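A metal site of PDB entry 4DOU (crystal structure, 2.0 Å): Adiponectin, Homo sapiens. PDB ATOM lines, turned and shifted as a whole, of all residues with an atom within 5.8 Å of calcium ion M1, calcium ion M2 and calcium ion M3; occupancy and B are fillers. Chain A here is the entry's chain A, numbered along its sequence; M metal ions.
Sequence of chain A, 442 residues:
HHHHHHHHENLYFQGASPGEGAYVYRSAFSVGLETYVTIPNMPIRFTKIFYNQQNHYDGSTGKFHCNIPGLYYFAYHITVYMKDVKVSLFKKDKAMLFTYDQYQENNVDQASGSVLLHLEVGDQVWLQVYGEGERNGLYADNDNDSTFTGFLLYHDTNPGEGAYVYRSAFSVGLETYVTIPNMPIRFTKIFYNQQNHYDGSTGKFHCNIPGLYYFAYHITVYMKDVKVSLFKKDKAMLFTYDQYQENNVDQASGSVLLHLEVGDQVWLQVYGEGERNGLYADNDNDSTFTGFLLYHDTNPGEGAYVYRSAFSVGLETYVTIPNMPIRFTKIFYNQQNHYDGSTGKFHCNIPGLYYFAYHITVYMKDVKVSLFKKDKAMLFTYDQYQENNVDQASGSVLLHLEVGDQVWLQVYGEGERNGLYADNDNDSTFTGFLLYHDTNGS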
ATOM      1  N   ASP A 101      21.382 -19.633 -27.316  1.00  0.00           N
ATOM      2  CA  ASP A 101      21.275 -19.871 -25.895  1.00  0.00           C
ATOM      3  C   ASP A 101      21.825 -21.275 -25.619  1.00  0.00           C
ATOM      4  O   ASP A 101      21.315 -22.262 -26.134  1.00  0.00           O
ATOM      5  CB  ASP A 101      19.812 -19.755 -25.443  1.00  0.00           C
ATOM      6  CG  ASP A 101      19.649 -19.561 -23.936  1.00  0.00           C
ATOM      7  OD1 ASP A 101      18.575 -19.082 -23.512  1.00  0.00           O
ATOM      8  OD2 ASP A 101      20.580 -19.906 -23.181  1.00  0.00           O
ATOM      9  N   GLN A 102      22.907 -21.339 -24.837  1.00  0.00           N
ATOM     10  CA  GLN A 102      23.540 -22.620 -24.521  1.00  0.00           C
ATOM     11  C   GLN A 102      22.787 -23.294 -23.379  1.00  0.00           C
ATOM     12  O   GLN A 102      22.222 -22.617 -22.514  1.00  0.00           O
ATOM     13  CB  GLN A 102      25.020 -22.428 -24.131  1.00  0.00           C
ATOM     14  CG  GLN A 102      25.975 -22.451 -25.315  1.00  0.00           C
ATOM     15  CD  GLN A 102      27.420 -22.171 -24.928  1.00  0.00           C
ATOM     16  OE1 GLN A 102      27.704 -21.259 -24.145  1.00  0.00           O
ATOM     17  NE2 GLN A 102      28.340 -22.943 -25.482  1.00  0.00           N
ATOM     18  N   TYR A 103      22.760 -24.622 -23.391  1.00  0.00           N
ATOM     19  CA  TYR A 103      22.115 -25.401 -22.350  1.00  0.00           C
ATOM     20  C   TYR A 103      23.146 -26.107 -21.469  1.00  0.00           C
ATOM     21  O   TYR A 103      24.103 -26.700 -21.959  1.00  0.00           O
ATOM     22  CB  TYR A 103      21.186 -26.463 -22.940  1.00  0.00           C
ATOM     23  CG  TYR A 103      20.582 -27.367 -21.882  1.00  0.00           C
ATOM     24  CD1 TYR A 103      19.556 -26.916 -21.081  1.00  0.00           C
ATOM     25  CD2 TYR A 103      21.066 -28.649 -21.681  1.00  0.00           C
ATOM     26  CE1 TYR A 103      19.008 -27.730 -20.097  1.00  0.00           C
ATOM     27  CE2 TYR A 103      20.527 -29.468 -20.699  1.00  0.00           C
ATOM     28  CZ  TYR A 103      19.495 -29.000 -19.915  1.00  0.00           C
ATOM     29  OH  TYR A 103      18.951 -29.803 -18.940  1.00  0.00           O
ATOM     30  N   ASN A 107      19.618 -27.263 -16.140  1.00  0.00           N
ATOM     31  CA  ASN A 107      19.465 -25.820 -16.190  1.00  0.00           C
ATOM     32  C   ASN A 107      18.638 -25.308 -17.379  1.00  0.00           C
ATOM     33  O   ASN A 107      19.159 -24.647 -18.273  1.00  0.00           O
ATOM     34  CB  ASN A 107      20.832 -25.156 -16.162  1.00  0.00           C
ATOM     35  CG  ASN A 107      20.748 -23.702 -15.770  1.00  0.00           C
ATOM     36  OD1 ASN A 107      19.704 -23.082 -15.908  1.00  0.00           O
ATOM     37  ND2 ASN A 107      21.849 -23.156 -15.271  1.00  0.00           N
ATOM     38  N   VAL A 108      17.348 -25.595 -17.368  1.00  0.00           N
ATOM     39  CA  VAL A 108      16.449 -25.105 -18.399  1.00  0.00           C
ATOM     40  C   VAL A 108      16.549 -23.585 -18.528  1.00  0.00           C
ATOM     41  O   VAL A 108      16.532 -22.852 -17.524  1.00  0.00           O
ATOM     42  CB  VAL A 108      15.001 -25.516 -18.113  1.00  0.00           C
ATOM     43  CG1 VAL A 108      14.041 -24.894 -19.107  1.00  0.00           C
ATOM     44  CG2 VAL A 108      14.892 -27.054 -18.099  1.00  0.00           C
ATOM     45  N   ASP A 109      16.642 -23.128 -19.781  1.00  0.00           N
ATOM     46  CA  ASP A 109      16.759 -21.703 -20.089  1.00  0.00           C
ATOM     47  C   ASP A 109      15.611 -21.133 -20.916  1.00  0.00           C
ATOM     48  O   ASP A 109      14.760 -21.867 -21.443  1.00  0.00           O
ATOM     49  CB  ASP A 109      18.091 -21.408 -20.777  1.00  0.00           C
ATOM     50  CG  ASP A 109      19.202 -21.234 -19.777  1.00  0.00           C
ATOM     51  OD1 ASP A 109      18.880 -21.050 -18.590  1.00  0.00           O
ATOM     52  OD2 ASP A 109      20.394 -21.279 -20.166  1.00  0.00           O
ATOM     53  N   GLN A 110      15.587 -19.811 -21.031  1.00  0.00           N
ATOM     54  CA  GLN A 110      14.593 -19.132 -21.828  1.00  0.00           C
ATOM     55  C   GLN A 110      15.269 -18.174 -22.774  1.00  0.00           C
ATOM     56  O   GLN A 110      15.971 -17.272 -22.336  1.00  0.00           O
ATOM     57  CB  GLN A 110      13.589 -18.380 -20.952  1.00  0.00           C
ATOM     58  CG  GLN A 110      12.619 -19.274 -20.217  1.00  0.00           C
ATOM     59  CD  GLN A 110      11.663 -19.993 -21.147  1.00  0.00           C
ATOM     60  OE1 GLN A 110      11.279 -21.154 -20.909  1.00  0.00           O
ATOM     61  NE2 GLN A 110      11.242 -19.301 -22.202  1.00  0.00           N
ATOM     62  N   ASP A 242      21.557 -10.351 -15.907  1.00  0.00           N
ATOM     63  CA  ASP A 242      21.672 -11.740 -16.313  1.00  0.00           C
ATOM     64  C   ASP A 242      23.093 -12.218 -16.084  1.00  0.00           C
ATOM     65  O   ASP A 242      24.043 -11.703 -16.683  1.00  0.00           O
ATOM     66  CB  ASP A 242      21.245 -11.918 -17.779  1.00  0.00           C
ATOM     67  CG  ASP A 242      20.946 -13.374 -18.138  1.00  0.00           C
ATOM     68  OD1 ASP A 242      21.395 -14.268 -17.393  1.00  0.00           O
ATOM     69  OD2 ASP A 242      20.255 -13.634 -19.159  1.00  0.00           O
ATOM     70  N   GLN A 243      23.241 -13.212 -15.218  1.00  0.00           N
ATOM     71  CA  GLN A 243      24.550 -13.694 -14.793  1.00  0.00           C
ATOM     72  C   GLN A 243      25.122 -14.681 -15.789  1.00  0.00           C
ATOM     73  O   GLN A 243      24.399 -15.515 -16.337  1.00  0.00           O
ATOM     74  CB  GLN A 243      24.459 -14.368 -13.422  1.00  0.00           C
ATOM     75  CG  GLN A 243      25.119 -13.613 -12.289  1.00  0.00           C
ATOM     76  CD  GLN A 243      25.182 -14.441 -11.010  1.00  0.00           C
ATOM     77  OE1 GLN A 243      24.183 -14.995 -10.564  1.00  0.00           O
ATOM     78  NE2 GLN A 243      26.368 -14.520 -10.415  1.00  0.00           N
ATOM     79  N   TYR A 244      26.431 -14.612 -16.001  1.00  0.00           N
ATOM     80  CA  TYR A 244      27.101 -15.510 -16.912  1.00  0.00           C
ATOM     81  C   TYR A 244      27.981 -16.529 -16.207  1.00  0.00           C
ATOM     82  O   TYR A 244      28.911 -16.175 -15.494  1.00  0.00           O
ATOM     83  CB  TYR A 244      27.957 -14.735 -17.918  1.00  0.00           C
ATOM     84  CG  TYR A 244      28.714 -15.657 -18.844  1.00  0.00           C
ATOM     85  CD1 TYR A 244      28.082 -16.214 -19.949  1.00  0.00           C
ATOM     86  CD2 TYR A 244      30.042 -15.981 -18.620  1.00  0.00           C
ATOM     87  CE1 TYR A 244      28.738 -17.055 -20.789  1.00  0.00           C
ATOM     88  CE2 TYR A 244      30.724 -16.836 -19.465  1.00  0.00           C
ATOM     89  CZ  TYR A 244      30.063 -17.368 -20.553  1.00  0.00           C
ATOM     90  OH  TYR A 244      30.690 -18.215 -21.411  1.00  0.00           O
ATOM     91  N   GLN A 245      27.678 -17.804 -16.424  1.00  0.00           N
ATOM     92  CA  GLN A 245      28.568 -18.860 -15.980  1.00  0.00           C
ATOM     93  C   GLN A 245      29.305 -19.401 -17.199  1.00  0.00           C
ATOM     94  O   GLN A 245      28.813 -19.302 -18.329  1.00  0.00           O
ATOM     95  CB  GLN A 245      27.812 -19.968 -15.272  1.00  0.00           C
ATOM     96  CG  GLN A 245      28.628 -20.627 -14.156  1.00  0.00           C
ATOM     97  CD  GLN A 245      28.557 -19.848 -12.853  1.00  0.00           C
ATOM     98  OE1 GLN A 245      29.575 -19.409 -12.321  1.00  0.00           O
ATOM     99  NE2 GLN A 245      27.345 -19.668 -12.339  1.00  0.00           N
ATOM    100  N   ASN A 248      28.130 -21.098 -20.725  1.00  0.00           N
ATOM    101  CA  ASN A 248      26.678 -20.983 -20.681  1.00  0.00           C
ATOM    102  C   ASN A 248      26.170 -19.645 -21.207  1.00  0.00           C
ATOM    103  O   ASN A 248      25.691 -18.813 -20.429  1.00  0.00           O
ATOM    104  CB  ASN A 248      26.152 -21.234 -19.265  1.00  0.00           C
ATOM    105  CG  ASN A 248      24.657 -21.505 -19.237  1.00  0.00           C
ATOM    106  OD1 ASN A 248      23.979 -21.453 -20.261  1.00  0.00           O
ATOM    107  ND2 ASN A 248      24.126 -21.789 -18.048  1.00  0.00           N
ATOM    108  N   VAL A 249      26.285 -19.434 -22.511  1.00  0.00           N
ATOM    109  CA  VAL A 249      25.742 -18.241 -23.126  1.00  0.00           C
ATOM    110  C   VAL A 249      24.258 -18.196 -22.765  1.00  0.00           C
ATOM    111  O   VAL A 249      23.560 -19.210 -22.773  1.00  0.00           O
ATOM    112  CB  VAL A 249      25.889 -18.251 -24.673  1.00  0.00           C
ATOM    113  CG1 VAL A 249      25.041 -17.132 -25.306  1.00  0.00           C
ATOM    114  CG2 VAL A 249      27.362 -18.136 -25.100  1.00  0.00           C
ATOM    115  N   ASP A 250      23.793 -17.000 -22.411  1.00  0.00           N
ATOM    116  CA  ASP A 250      22.407 -16.809 -21.996  1.00  0.00           C
ATOM    117  C   ASP A 250      21.739 -15.740 -22.861  1.00  0.00           C
ATOM    118  O   ASP A 250      22.403 -15.073 -23.678  1.00  0.00           O
ATOM    119  CB  ASP A 250      22.344 -16.393 -20.507  1.00  0.00           C
ATOM    120  CG  ASP A 250      22.355 -17.595 -19.557  1.00  0.00           C
ATOM    121  OD1 ASP A 250      22.692 -17.424 -18.356  1.00  0.00           O
ATOM    122  OD2 ASP A 250      22.020 -18.719 -19.981  1.00  0.00           O
ATOM    123  N   GLN A 251      20.434 -15.592 -22.677  1.00  0.00           N
ATOM    124  CA  GLN A 251      19.653 -14.582 -23.375  1.00  0.00           C
ATOM    125  C   GLN A 251      18.811 -13.802 -22.391  1.00  0.00           C
ATOM    126  O   GLN A 251      18.103 -14.378 -21.565  1.00  0.00           O
ATOM    127  CB  GLN A 251      18.736 -15.255 -24.405  1.00  0.00           C
ATOM    128  CG  GLN A 251      19.471 -15.832 -25.599  1.00  0.00           C
ATOM    129  CD  GLN A 251      20.021 -14.775 -26.515  1.00  0.00           C
ATOM    130  OE1 GLN A 251      20.907 -15.048 -27.333  1.00  0.00           O
ATOM    131  NE2 GLN A 251      19.477 -13.547 -26.412  1.00  0.00           N
ATOM    132  N   VAL A 362      15.125 -14.392 -12.563  1.00  0.00           N
ATOM    133  CA  VAL A 362      15.085 -15.717 -11.952  1.00  0.00           C
ATOM    134  C   VAL A 362      16.219 -15.829 -10.949  1.00  0.00           C
ATOM    135  O   VAL A 362      17.385 -15.884 -11.327  1.00  0.00           O
ATOM    136  CB  VAL A 362      15.215 -16.800 -13.024  1.00  0.00           C
ATOM    137  CG1 VAL A 362      15.100 -18.211 -12.398  1.00  0.00           C
ATOM    138  CG2 VAL A 362      14.174 -16.579 -14.133  1.00  0.00           C
ATOM    139  N   ASP A 383      11.833 -21.726 -16.131  1.00  0.00           N
ATOM    140  CA  ASP A 383      13.247 -21.366 -16.166  1.00  0.00           C
ATOM    141  C   ASP A 383      13.959 -21.826 -14.884  1.00  0.00           C
ATOM    142  O   ASP A 383      13.738 -21.298 -13.798  1.00  0.00           O
ATOM    143  CB  ASP A 383      13.421 -19.851 -16.426  1.00  0.00           C
ATOM    144  CG  ASP A 383      14.832 -19.495 -16.879  1.00  0.00           C
ATOM    145  OD1 ASP A 383      15.735 -20.355 -16.763  1.00  0.00           O
ATOM    146  OD2 ASP A 383      15.033 -18.349 -17.364  1.00  0.00           O
ATOM    147  N   GLN A 384      14.812 -22.839 -15.030  1.00  0.00           N
ATOM    148  CA  GLN A 384      15.526 -23.379 -13.873  1.00  0.00           C
ATOM    149  C   GLN A 384      16.570 -22.409 -13.331  1.00  0.00           C
ATOM    150  O   GLN A 384      17.098 -21.574 -14.066  1.00  0.00           O
ATOM    151  CB  GLN A 384      16.169 -24.716 -14.230  1.00  0.00           C
ATOM    152  CG  GLN A 384      15.276 -25.903 -13.957  1.00  0.00           C
ATOM    153  CD  GLN A 384      15.984 -27.221 -14.155  1.00  0.00           C
ATOM    154  OE1 GLN A 384      16.459 -27.518 -15.255  1.00  0.00           O
ATOM    155  NE2 GLN A 384      16.053 -28.020 -13.097  1.00  0.00           N
ATOM    156  N   TYR A 385      16.843 -22.508 -12.034  1.00  0.00           N
ATOM    157  CA  TYR A 385      17.862 -21.656 -11.426  1.00  0.00           C
ATOM    158  C   TYR A 385      19.036 -22.502 -10.961  1.00  0.00           C
ATOM    159  O   TYR A 385      18.844 -23.522 -10.295  1.00  0.00           O
ATOM    160  CB  TYR A 385      17.299 -20.852 -10.246  1.00  0.00           C
ATOM    161  CG  TYR A 385      18.366 -20.034  -9.537  1.00  0.00           C
ATOM    162  CD1 TYR A 385      18.777 -18.806 -10.043  1.00  0.00           C
ATOM    163  CD2 TYR A 385      18.975 -20.496  -8.365  1.00  0.00           C
ATOM    164  CE1 TYR A 385      19.758 -18.060  -9.406  1.00  0.00           C
ATOM    165  CE2 TYR A 385      19.956 -19.752  -7.719  1.00  0.00           C
ATOM    166  CZ  TYR A 385      20.341 -18.541  -8.256  1.00  0.00           C
ATOM    167  OH  TYR A 385      21.312 -17.790  -7.627  1.00  0.00           O
ATOM    168  N   GLN A 386      20.231 -22.082 -11.338  1.00  0.00           N
ATOM    169  CA  GLN A 386      21.454 -22.698 -10.823  1.00  0.00           C
ATOM    170  C   GLN A 386      22.205 -21.693  -9.946  1.00  0.00           C
ATOM    171  O   GLN A 386      22.277 -20.503 -10.276  1.00  0.00           O
ATOM    172  CB  GLN A 386      22.336 -23.210 -11.963  1.00  0.00           C
ATOM    173  CG  GLN A 386      23.531 -24.031 -11.517  1.00  0.00           C
ATOM    174  CD  GLN A 386      24.198 -24.805 -12.653  1.00  0.00           C
ATOM    175  OE1 GLN A 386      23.709 -24.809 -13.790  1.00  0.00           O
ATOM    176  NE2 GLN A 386      25.323 -25.461 -12.357  1.00  0.00           N
ATOM    177  N   ASN A 389      23.778 -18.093 -10.680  1.00  0.00           N
ATOM    178  CA  ASN A 389      23.396 -17.879 -12.080  1.00  0.00           C
ATOM    179  C   ASN A 389      21.999 -17.297 -12.224  1.00  0.00           C
ATOM    180  O   ASN A 389      21.088 -17.985 -12.656  1.00  0.00           O
ATOM    181  CB  ASN A 389      23.522 -19.179 -12.890  1.00  0.00           C
ATOM    182  CG  ASN A 389      23.502 -18.933 -14.398  1.00  0.00           C
ATOM    183  OD1 ASN A 389      23.123 -17.853 -14.867  1.00  0.00           O
ATOM    184  ND2 ASN A 389      23.903 -19.941 -15.164  1.00  0.00           N
ATOM    185  N   VAL A 390      21.838 -16.027 -11.853  1.00  0.00           N
ATOM    186  CA  VAL A 390      20.600 -15.313 -12.127  1.00  0.00           C
ATOM    187  C   VAL A 390      20.271 -15.496 -13.605  1.00  0.00           C
ATOM    188  O   VAL A 390      21.171 -15.465 -14.458  1.00  0.00           O
ATOM    189  CB  VAL A 390      20.728 -13.817 -11.814  1.00  0.00           C
ATOM    190  CG1 VAL A 390      19.576 -13.025 -12.433  1.00  0.00           C
ATOM    191  CG2 VAL A 390      20.796 -13.600 -10.300  1.00  0.00           C
ATOM    192  N   ASP A 391      18.990 -15.691 -13.906  1.00  0.00           N
ATOM    193  CA  ASP A 391      18.494 -15.863 -15.272  1.00  0.00           C
ATOM    194  C   ASP A 391      17.364 -14.893 -15.610  1.00  0.00           C
ATOM    195  O   ASP A 391      16.745 -14.281 -14.729  1.00  0.00           O
ATOM    196  CB  ASP A 391      18.017 -17.294 -15.494  1.00  0.00           C
ATOM    197  CG  ASP A 391      19.116 -18.230 -15.931  1.00  0.00           C
ATOM    198  OD1 ASP A 391      20.198 -17.729 -16.283  1.00  0.00           O
ATOM    199  OD2 ASP A 391      18.900 -19.457 -15.947  1.00  0.00           O
ATOM    200  N   GLN A 392      17.082 -14.789 -16.906  1.00  0.00           N
ATOM    201  CA  GLN A 392      16.008 -13.959 -17.405  1.00  0.00           C
ATOM    202  C   GLN A 392      15.072 -14.798 -18.265  1.00  0.00           C
ATOM    203  O   GLN A 392      15.492 -15.395 -19.264  1.00  0.00           O
ATOM    204  CB  GLN A 392      16.554 -12.805 -18.244  1.00  0.00           C
ATOM    205  CG  GLN A 392      17.214 -11.711 -17.425  1.00  0.00           C
ATOM    206  CD  GLN A 392      16.241 -10.919 -16.556  1.00  0.00           C
ATOM    207  OE1 GLN A 392      15.056 -10.764 -16.884  1.00  0.00           O
ATOM    208  NE2 GLN A 392      16.752 -10.400 -15.442  1.00  0.00           N
HETATM  209 CA    CA M   1      22.138 -16.230 -16.413  1.00  0.00          CA
HETATM  210 CA    CA M   2      17.810 -21.346 -16.394  1.00  0.00          CA
HETATM  211 CA    CA M   3      22.093 -20.407 -21.437  1.00  0.00          CA
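Within 4 Å of calcium ion M3: Asp 101, Gln 102, Asp 109, Asn 248, Val 249 and Asp 250.
The nearest printed residue that does not touch calcium ion M3 is Tyr 103 (4.7 Å).
Calcium ion M3 is bound by the side-chain carboxylate (OD2) of Asp 250 (2.2 Å), the side-chain carboxylate (OD2) of Asp 109 (2.3 Å), the backbone carbonyl oxygen (O) of Val 249 (2.3 Å), the side-chain carboxylate (OD2) of Asp 101 (2.4 Å), the side-chain amide oxygen (OD1) of Asn 248 (2.5 Å) and the backbone carbonyl oxygen (O) of Gln 102 (2.5 Å).
Calcium ion M3 has six donor atoms within binding distance.
Of the 24 residues printed, 6 come within 4 Å of calcium ion M2.
Calcium ion M2 is bound by the side-chain carboxylate (OD2) of Asp 391.
Calcium ion M2 is bound by O of Val 108 (2.3 Å).
Calcium ion M2 is bound by the side-chain carboxylate (OD1) of Asp 383, at 2.3 Å.
O of Gln 384 is bound to calcium ion M2 (2.4 Å).
The side-chain carboxylate (OD1) of Asp 109 binds calcium ion M2, 2.5 Å away.
Calcium ion M2 is bound by OD1 of Asn 107.
Calcium ion M2 has six donor atoms within binding distance.
Along chain A the residues within 4 Å of calcium ion M1 span positions 242 to 391.
The nearest printed residue that does not touch calcium ion M1 is Tyr 244 (4.6 Å).
ND2 of Asn 107 lies within hydrogen-bond range of OE1 of Gln 386 (2.9 Å).
ND2 of Asn 389 sits close to ND2 of Asn 248 (3.4 Å).
The backbone NH (N) of Val 362 lies within hydrogen-bond range of the backbone carbonyl oxygen (O) of Asp 391 (2.7 Å).
Calcium ion M1 is bound by O of Val 390 (2.3 Å).
Calcium ion M1 is bound by OD1 of Asp 242.
The side-chain carboxylate (OD1) of Asp 250 is bound to calcium ion M1, 2.3 Å away.
Calcium ion M1 is bound by O of Gln 243 (2.4 Å).
OD1 of Asn 389 binds calcium ion M1 (2.4 Å).
Calcium ion M1 is bound by OD1 of Asp 391 (2.5 Å).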
